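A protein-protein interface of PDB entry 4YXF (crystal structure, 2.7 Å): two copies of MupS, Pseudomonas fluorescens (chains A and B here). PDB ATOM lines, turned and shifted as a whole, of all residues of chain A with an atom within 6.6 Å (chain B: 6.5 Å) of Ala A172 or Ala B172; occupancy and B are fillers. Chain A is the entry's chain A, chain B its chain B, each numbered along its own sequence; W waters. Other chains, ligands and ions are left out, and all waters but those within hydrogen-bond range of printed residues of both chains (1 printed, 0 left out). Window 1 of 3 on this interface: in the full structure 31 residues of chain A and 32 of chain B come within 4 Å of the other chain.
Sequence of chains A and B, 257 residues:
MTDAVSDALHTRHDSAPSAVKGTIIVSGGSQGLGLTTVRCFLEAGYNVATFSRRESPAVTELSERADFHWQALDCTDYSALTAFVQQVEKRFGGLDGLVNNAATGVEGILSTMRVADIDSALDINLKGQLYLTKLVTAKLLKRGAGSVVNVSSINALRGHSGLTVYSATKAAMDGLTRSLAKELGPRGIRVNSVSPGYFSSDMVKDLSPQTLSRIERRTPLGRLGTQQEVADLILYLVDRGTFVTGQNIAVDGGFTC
Among the printed residues, merely in contact across the chains: Leu A122 with Leu B126, Thr A164 with Leu B176, Ala A171 with Ala B171, Ala A168 with Ala B172, Ala A172 with Ala B168, Leu A126 with Leu B126, Gly A175 with Ala B171, Ala A171 with Gly B175, Leu A176 with Thr B164, Ala A172 with Ala B172, Ser A167 with Gly B175 and Gly A175 with Ser B167.
Ala B172 touches two residues of chain A. Printed residues of chain B within 4 Å of Thr A164: Leu B176. Of the printed residues of chain B, Ala A171 touches Ala B171 and Gly B175. Of the printed residues of chain B, Ser A167 touches Gly B175 (3.8 Å). The nearest printed residue of chain A that does not touch Leu B176 is Ala A168 (4.4 Å).
Hydrophobic or aromatic side chains of chain B within 4 Å of the printed part of chain A: Leu B126, Ala B168, Ala B171, Ala B172 and Leu B176. Of the 15 printed residues of chain A, 9 touch a printed residue of chain B. Hydrophobic or aromatic side chains of chain A that line the printed part of chain B: Leu A122, Leu A126, Ala A168, Ala A171, Ala A172 and Leu A176. Among the printed residues, 12 pairs touch across the chains.
Leu B126 touches its own counterpart, Leu A126. Ala A168 touches Ala B172, and with the chains exchanged Ala A172 touches Ala B168. Ala A171 touches its own counterpart, Ala B171. Ala A171 touches Gly B175, and with the chains exchanged Gly A175 touches Ala B171.
Water W1 bridges the backbone carbonyl oxygen of Gly B175 (3.1 Å) and the backbone carbonyl oxygen of Ala A156 (3.3 Å).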
ATOM      1  N   LEU A 122     -18.609  17.467  36.751  1.00  0.00           N
ATOM      2  CA  LEU A 122     -19.537  17.918  35.725  1.00  0.00           C
ATOM      3  C   LEU A 122     -20.947  18.211  36.249  1.00  0.00           C
ATOM      4  O   LEU A 122     -21.555  19.190  35.829  1.00  0.00           O
ATOM      5  CB  LEU A 122     -19.620  16.920  34.587  1.00  0.00           C
ATOM      6  CG  LEU A 122     -18.430  16.636  33.706  1.00  0.00           C
ATOM      7  CD1 LEU A 122     -18.695  15.512  32.738  1.00  0.00           C
ATOM      8  CD2 LEU A 122     -18.244  17.936  32.960  1.00  0.00           C
ATOM      9  N   LEU A 126     -21.463  22.198  36.267  1.00  0.00           N
ATOM     10  CA  LEU A 126     -21.880  22.515  34.902  1.00  0.00           C
ATOM     11  C   LEU A 126     -23.358  22.262  34.654  1.00  0.00           C
ATOM     12  O   LEU A 126     -24.053  23.081  34.053  1.00  0.00           O
ATOM     13  CB  LEU A 126     -21.039  21.729  33.894  1.00  0.00           C
ATOM     14  CG  LEU A 126     -21.400  21.917  32.418  1.00  0.00           C
ATOM     15  CD1 LEU A 126     -21.387  23.391  32.045  1.00  0.00           C
ATOM     16  CD2 LEU A 126     -20.453  21.125  31.528  1.00  0.00           C
ATOM     17  N   ALA A 156     -10.367  29.706  33.289  1.00  0.00           N
ATOM     18  CA  ALA A 156     -11.085  29.401  32.088  1.00  0.00           C
ATOM     19  C   ALA A 156     -10.449  30.108  30.905  1.00  0.00           C
ATOM     20  O   ALA A 156     -10.703  29.727  29.743  1.00  0.00           O
ATOM     21  CB  ALA A 156     -12.502  29.810  32.253  1.00  0.00           C
ATOM     22  N   THR A 164      -7.485  21.077  35.372  1.00  0.00           N
ATOM     23  CA  THR A 164      -7.972  20.510  34.169  1.00  0.00           C
ATOM     24  C   THR A 164      -9.465  20.432  34.027  1.00  0.00           C
ATOM     25  O   THR A 164     -10.011  20.989  33.147  1.00  0.00           O
ATOM     26  CB  THR A 164      -7.374  19.127  34.049  1.00  0.00           C
ATOM     27  OG1 THR A 164      -5.968  19.254  33.995  1.00  0.00           O
ATOM     28  CG2 THR A 164      -7.811  18.500  32.837  1.00  0.00           C
ATOM     29  N   SER A 167     -11.287  23.785  34.849  1.00  0.00           N
ATOM     30  CA  SER A 167     -11.168  24.718  33.755  1.00  0.00           C
ATOM     31  C   SER A 167     -12.199  24.396  32.652  1.00  0.00           C
ATOM     32  O   SER A 167     -12.794  25.301  32.047  1.00  0.00           O
ATOM     33  CB  SER A 167      -9.754  24.631  33.185  1.00  0.00           C
ATOM     34  OG  SER A 167      -8.821  25.097  34.147  1.00  0.00           O
ATOM     35  N   ALA A 168     -12.405  23.103  32.400  1.00  0.00           N
ATOM     36  CA  ALA A 168     -13.417  22.705  31.442  1.00  0.00           C
ATOM     37  C   ALA A 168     -14.774  23.244  31.875  1.00  0.00           C
ATOM     38  O   ALA A 168     -15.472  23.865  31.103  1.00  0.00           O
ATOM     39  CB  ALA A 168     -13.464  21.187  31.292  1.00  0.00           C
ATOM     40  N   THR A 169     -15.142  23.047  33.122  1.00  0.00           N
ATOM     41  CA  THR A 169     -16.496  23.423  33.500  1.00  0.00           C
ATOM     42  C   THR A 169     -16.669  24.957  33.475  1.00  0.00           C
ATOM     43  O   THR A 169     -17.766  25.468  33.085  1.00  0.00           O
ATOM     44  CB  THR A 169     -16.929  22.818  34.848  1.00  0.00           C
ATOM     45  OG1 THR A 169     -15.940  23.162  35.819  1.00  0.00           O
ATOM     46  CG2 THR A 169     -17.023  21.300  34.740  1.00  0.00           C
ATOM     47  N   LYS A 170     -15.604  25.688  33.815  1.00  0.00           N
ATOM     48  CA  LYS A 170     -15.720  27.133  33.800  1.00  0.00           C
ATOM     49  C   LYS A 170     -15.722  27.658  32.375  1.00  0.00           C
ATOM     50  O   LYS A 170     -16.530  28.481  31.994  1.00  0.00           O
ATOM     51  CB  LYS A 170     -14.641  27.777  34.630  1.00  0.00           C
ATOM     52  CG  LYS A 170     -14.822  27.554  36.123  1.00  0.00           C
ATOM     53  CD  LYS A 170     -16.246  27.854  36.614  1.00  0.00           C
ATOM     54  CE  LYS A 170     -16.225  28.023  38.127  1.00  0.00           C
ATOM     55  NZ  LYS A 170     -17.012  29.169  38.664  1.00  0.00           N
ATOM     56  N   ALA A 171     -14.864  27.121  31.545  1.00  0.00           N
ATOM     57  CA  ALA A 171     -14.827  27.588  30.176  1.00  0.00           C
ATOM     58  C   ALA A 171     -16.141  27.199  29.504  1.00  0.00           C
ATOM     59  O   ALA A 171     -16.501  27.716  28.437  1.00  0.00           O
ATOM     60  CB  ALA A 171     -13.618  27.000  29.442  1.00  0.00           C
ATOM     61  N   ALA A 172     -16.863  26.271  30.061  1.00  0.00           N
ATOM     62  CA  ALA A 172     -18.079  25.842  29.437  1.00  0.00           C
ATOM     63  C   ALA A 172     -19.122  26.883  29.624  1.00  0.00           C
ATOM     64  O   ALA A 172     -19.874  27.176  28.758  1.00  0.00           O
ATOM     65  CB  ALA A 172     -18.526  24.557  30.055  1.00  0.00           C
ATOM     66  N   MET A 173     -19.143  27.457  30.790  1.00  0.00           N
ATOM     67  CA  MET A 173     -20.097  28.479  31.049  1.00  0.00           C
ATOM     68  C   MET A 173     -19.780  29.716  30.274  1.00  0.00           C
ATOM     69  O   MET A 173     -20.660  30.452  29.922  1.00  0.00           O
ATOM     70  CB  MET A 173     -20.142  28.775  32.529  1.00  0.00           C
ATOM     71  CG  MET A 173     -20.662  27.630  33.359  1.00  0.00           C
ATOM     72  SD  MET A 173     -22.320  27.142  32.932  1.00  0.00           S
ATOM     73  CE  MET A 173     -23.203  28.574  33.448  1.00  0.00           C
ATOM     74  N   ASP A 174     -18.509  29.941  30.006  1.00  0.00           N
ATOM     75  CA  ASP A 174     -18.133  31.059  29.152  1.00  0.00           C
ATOM     76  C   ASP A 174     -18.510  30.829  27.710  1.00  0.00           C
ATOM     77  O   ASP A 174     -18.742  31.783  27.004  1.00  0.00           O
ATOM     78  CB  ASP A 174     -16.690  31.435  29.358  1.00  0.00           C
ATOM     79  CG  ASP A 174     -16.419  31.874  30.818  1.00  0.00           C
ATOM     80  OD1 ASP A 174     -15.236  31.800  31.279  1.00  0.00           O
ATOM     81  OD2 ASP A 174     -17.411  32.290  31.512  1.00  0.00           O
ATOM     82  N   GLY A 175     -18.694  29.566  27.314  1.00  0.00           N
ATOM     83  CA  GLY A 175     -19.134  29.244  25.989  1.00  0.00           C
ATOM     84  C   GLY A 175     -20.634  29.471  26.034  1.00  0.00           C
ATOM     85  O   GLY A 175     -21.234  29.951  25.088  1.00  0.00           O
ATOM     86  N   LEU A 176     -21.258  29.146  27.150  1.00  0.00           N
ATOM     87  CA  LEU A 176     -22.694  29.279  27.211  1.00  0.00           C
ATOM     88  C   LEU A 176     -23.048  30.754  27.145  1.00  0.00           C
ATOM     89  O   LEU A 176     -24.071  31.137  26.586  1.00  0.00           O
ATOM     90  CB  LEU A 176     -23.263  28.653  28.494  1.00  0.00           C
ATOM     91  CG  LEU A 176     -24.779  28.680  28.336  1.00  0.00           C
ATOM     92  CD1 LEU A 176     -25.380  27.478  29.023  1.00  0.00           C
ATOM     93  CD2 LEU A 176     -25.400  29.959  28.839  1.00  0.00           C
ATOM     94  N   THR A 177     -22.195  31.593  27.709  1.00  0.00           N
ATOM     95  CA  THR A 177     -22.508  33.005  27.735  1.00  0.00           C
ATOM     96  C   THR A 177     -22.549  33.543  26.334  1.00  0.00           C
ATOM     97  O   THR A 177     -23.401  34.338  26.004  1.00  0.00           O
ATOM     98  CB  THR A 177     -21.438  33.778  28.474  1.00  0.00           C
ATOM     99  OG1 THR A 177     -21.664  33.604  29.851  1.00  0.00           O
ATOM    100  CG2 THR A 177     -21.457  35.225  28.137  1.00  0.00           C
ATOM    101  N   LEU B 126     -19.031  15.521  26.287  1.00  0.00           N
ATOM    102  CA  LEU B 126     -18.039  16.059  27.192  1.00  0.00           C
ATOM    103  C   LEU B 126     -17.380  15.030  28.116  1.00  0.00           C
ATOM    104  O   LEU B 126     -16.163  14.963  28.183  1.00  0.00           O
ATOM    105  CB  LEU B 126     -18.502  17.372  27.890  1.00  0.00           C
ATOM    106  CG  LEU B 126     -17.547  17.877  28.992  1.00  0.00           C
ATOM    107  CD1 LEU B 126     -16.222  18.463  28.518  1.00  0.00           C
ATOM    108  CD2 LEU B 126     -18.224  18.857  29.931  1.00  0.00           C
ATOM    109  N   ALA B 156     -17.542  27.443  19.699  1.00  0.00           N
ATOM    110  CA  ALA B 156     -16.970  27.640  21.027  1.00  0.00           C
ATOM    111  C   ALA B 156     -16.304  29.000  21.108  1.00  0.00           C
ATOM    112  O   ALA B 156     -15.909  29.441  22.197  1.00  0.00           O
ATOM    113  CB  ALA B 156     -15.994  26.554  21.346  1.00  0.00           C
ATOM    114  N   THR B 164     -26.573  26.607  22.334  1.00  0.00           N
ATOM    115  CA  THR B 164     -26.163  26.813  23.718  1.00  0.00           C
ATOM    116  C   THR B 164     -25.374  25.639  24.293  1.00  0.00           C
ATOM    117  O   THR B 164     -24.173  25.755  24.535  1.00  0.00           O
ATOM    118  CB  THR B 164     -27.375  27.093  24.627  1.00  0.00           C
ATOM    119  OG1 THR B 164     -27.144  26.527  25.923  1.00  0.00           O
ATOM    120  CG2 THR B 164     -28.637  26.490  24.032  1.00  0.00           C
ATOM    121  N   SER B 167     -22.325  24.598  22.462  1.00  0.00           N
ATOM    122  CA  SER B 167     -21.245  25.591  22.604  1.00  0.00           C
ATOM    123  C   SER B 167     -20.623  25.397  23.946  1.00  0.00           C
ATOM    124  O   SER B 167     -19.418  25.465  24.070  1.00  0.00           O
ATOM    125  CB  SER B 167     -21.767  27.001  22.549  1.00  0.00           C
ATOM    126  OG  SER B 167     -22.155  27.340  21.237  1.00  0.00           O
ATOM    127  N   ALA B 168     -21.435  25.173  24.970  1.00  0.00           N
ATOM    128  CA  ALA B 168     -20.838  24.872  26.249  1.00  0.00           C
ATOM    129  C   ALA B 168     -19.902  23.664  26.159  1.00  0.00           C
ATOM    130  O   ALA B 168     -18.719  23.762  26.549  1.00  0.00           O
ATOM    131  CB  ALA B 168     -21.886  24.669  27.320  1.00  0.00           C
ATOM    132  N   THR B 169     -20.378  22.540  25.637  1.00  0.00           N
ATOM    133  CA  THR B 169     -19.478  21.373  25.604  1.00  0.00           C
ATOM    134  C   THR B 169     -18.255  21.591  24.735  1.00  0.00           C
ATOM    135  O   THR B 169     -17.163  21.195  25.131  1.00  0.00           O
ATOM    136  CB  THR B 169     -20.129  20.114  25.093  1.00  0.00           C
ATOM    137  OG1 THR B 169     -20.583  20.362  23.745  1.00  0.00           O
ATOM    138  CG2 THR B 169     -21.237  19.669  26.047  1.00  0.00           C
ATOM    139  N   LYS B 170     -18.405  22.222  23.572  1.00  0.00           N
ATOM    140  CA  LYS B 170     -17.195  22.620  22.792  1.00  0.00           C
ATOM    141  C   LYS B 170     -16.264  23.563  23.528  1.00  0.00           C
ATOM    142  O   LYS B 170     -15.058  23.426  23.476  1.00  0.00           O
ATOM    143  CB  LYS B 170     -17.509  23.168  21.394  1.00  0.00           C
ATOM    144  CG  LYS B 170     -17.970  22.053  20.472  1.00  0.00           C
ATOM    145  CD  LYS B 170     -17.645  20.722  21.125  1.00  0.00           C
ATOM    146  CE  LYS B 170     -17.629  19.574  20.147  1.00  0.00           C
ATOM    147  NZ  LYS B 170     -16.819  19.934  18.963  1.00  0.00           N
ATOM    148  N   ALA B 171     -16.793  24.527  24.235  1.00  0.00           N
ATOM    149  CA  ALA B 171     -15.887  25.496  24.819  1.00  0.00           C
ATOM    150  C   ALA B 171     -15.262  24.824  26.063  1.00  0.00           C
ATOM    151  O   ALA B 171     -14.153  25.176  26.462  1.00  0.00           O
ATOM    152  CB  ALA B 171     -16.615  26.774  25.150  1.00  0.00           C
ATOM    153  N   ALA B 172     -15.935  23.808  26.619  1.00  0.00           N
ATOM    154  CA  ALA B 172     -15.344  23.043  27.726  1.00  0.00           C
ATOM    155  C   ALA B 172     -14.031  22.401  27.304  1.00  0.00           C
ATOM    156  O   ALA B 172     -12.993  22.604  27.932  1.00  0.00           O
ATOM    157  CB  ALA B 172     -16.314  22.031  28.300  1.00  0.00           C
ATOM    158  N   MET B 173     -14.056  21.711  26.170  1.00  0.00           N
ATOM    159  CA  MET B 173     -12.842  21.136  25.600  1.00  0.00           C
ATOM    160  C   MET B 173     -11.772  22.091  25.054  1.00  0.00           C
ATOM    161  O   MET B 173     -10.748  21.640  24.541  1.00  0.00           O
ATOM    162  CB  MET B 173     -13.149  20.477  24.253  1.00  0.00           C
ATOM    163  CG  MET B 173     -12.398  19.178  24.011  1.00  0.00           C
ATOM    164  SD  MET B 173     -11.856  18.393  25.541  1.00  0.00           S
ATOM    165  CE  MET B 173     -13.347  17.525  26.024  1.00  0.00           C
ATOM    166  N   ASP B 174     -12.002  23.401  25.150  1.00  0.00           N
ATOM    167  CA  ASP B 174     -10.944  24.397  24.888  1.00  0.00           C
ATOM    168  C   ASP B 174     -10.332  24.910  26.191  1.00  0.00           C
ATOM    169  O   ASP B 174      -9.204  25.378  26.213  1.00  0.00           O
ATOM    170  CB  ASP B 174     -11.475  25.519  23.979  1.00  0.00           C
ATOM    171  CG  ASP B 174     -11.894  24.998  22.563  1.00  0.00           C
ATOM    172  OD1 ASP B 174     -11.655  23.791  22.278  1.00  0.00           O
ATOM    173  OD2 ASP B 174     -12.448  25.765  21.714  1.00  0.00           O
ATOM    174  N   GLY B 175     -11.081  24.787  27.287  1.00  0.00           N
ATOM    175  CA  GLY B 175     -10.576  25.226  28.550  1.00  0.00           C
ATOM    176  C   GLY B 175      -9.628  24.133  28.979  1.00  0.00           C
ATOM    177  O   GLY B 175      -8.575  24.386  29.553  1.00  0.00           O
ATOM    178  N   LEU B 176     -10.037  22.907  28.697  1.00  0.00           N
ATOM    179  CA  LEU B 176      -9.236  21.778  28.956  1.00  0.00           C
ATOM    180  C   LEU B 176      -7.932  21.899  28.193  1.00  0.00           C
ATOM    181  O   LEU B 176      -6.877  21.812  28.822  1.00  0.00           O
ATOM    182  CB  LEU B 176      -9.962  20.507  28.571  1.00  0.00           C
ATOM    183  CG  LEU B 176      -9.134  19.267  28.886  1.00  0.00           C
ATOM    184  CD1 LEU B 176      -9.625  18.812  30.233  1.00  0.00           C
ATOM    185  CD2 LEU B 176      -9.386  18.162  27.873  1.00  0.00           C
ATOM    186  N   THR B 177      -7.990  22.079  26.865  1.00  0.00           N
ATOM    187  CA  THR B 177      -6.773  22.233  26.104  1.00  0.00           C
ATOM    188  C   THR B 177      -5.741  23.126  26.825  1.00  0.00           C
ATOM    189  O   THR B 177      -4.571  22.706  26.997  1.00  0.00           O
ATOM    190  CB  THR B 177      -7.042  22.863  24.733  1.00  0.00           C
ATOM    191  OG1 THR B 177      -7.739  21.930  23.899  1.00  0.00           O
ATOM    192  CG2 THR B 177      -5.725  23.355  24.023  1.00  0.00           C
HETATM  193  O   HOH W   1      -8.435  27.435  30.175  1.00  0.00           O
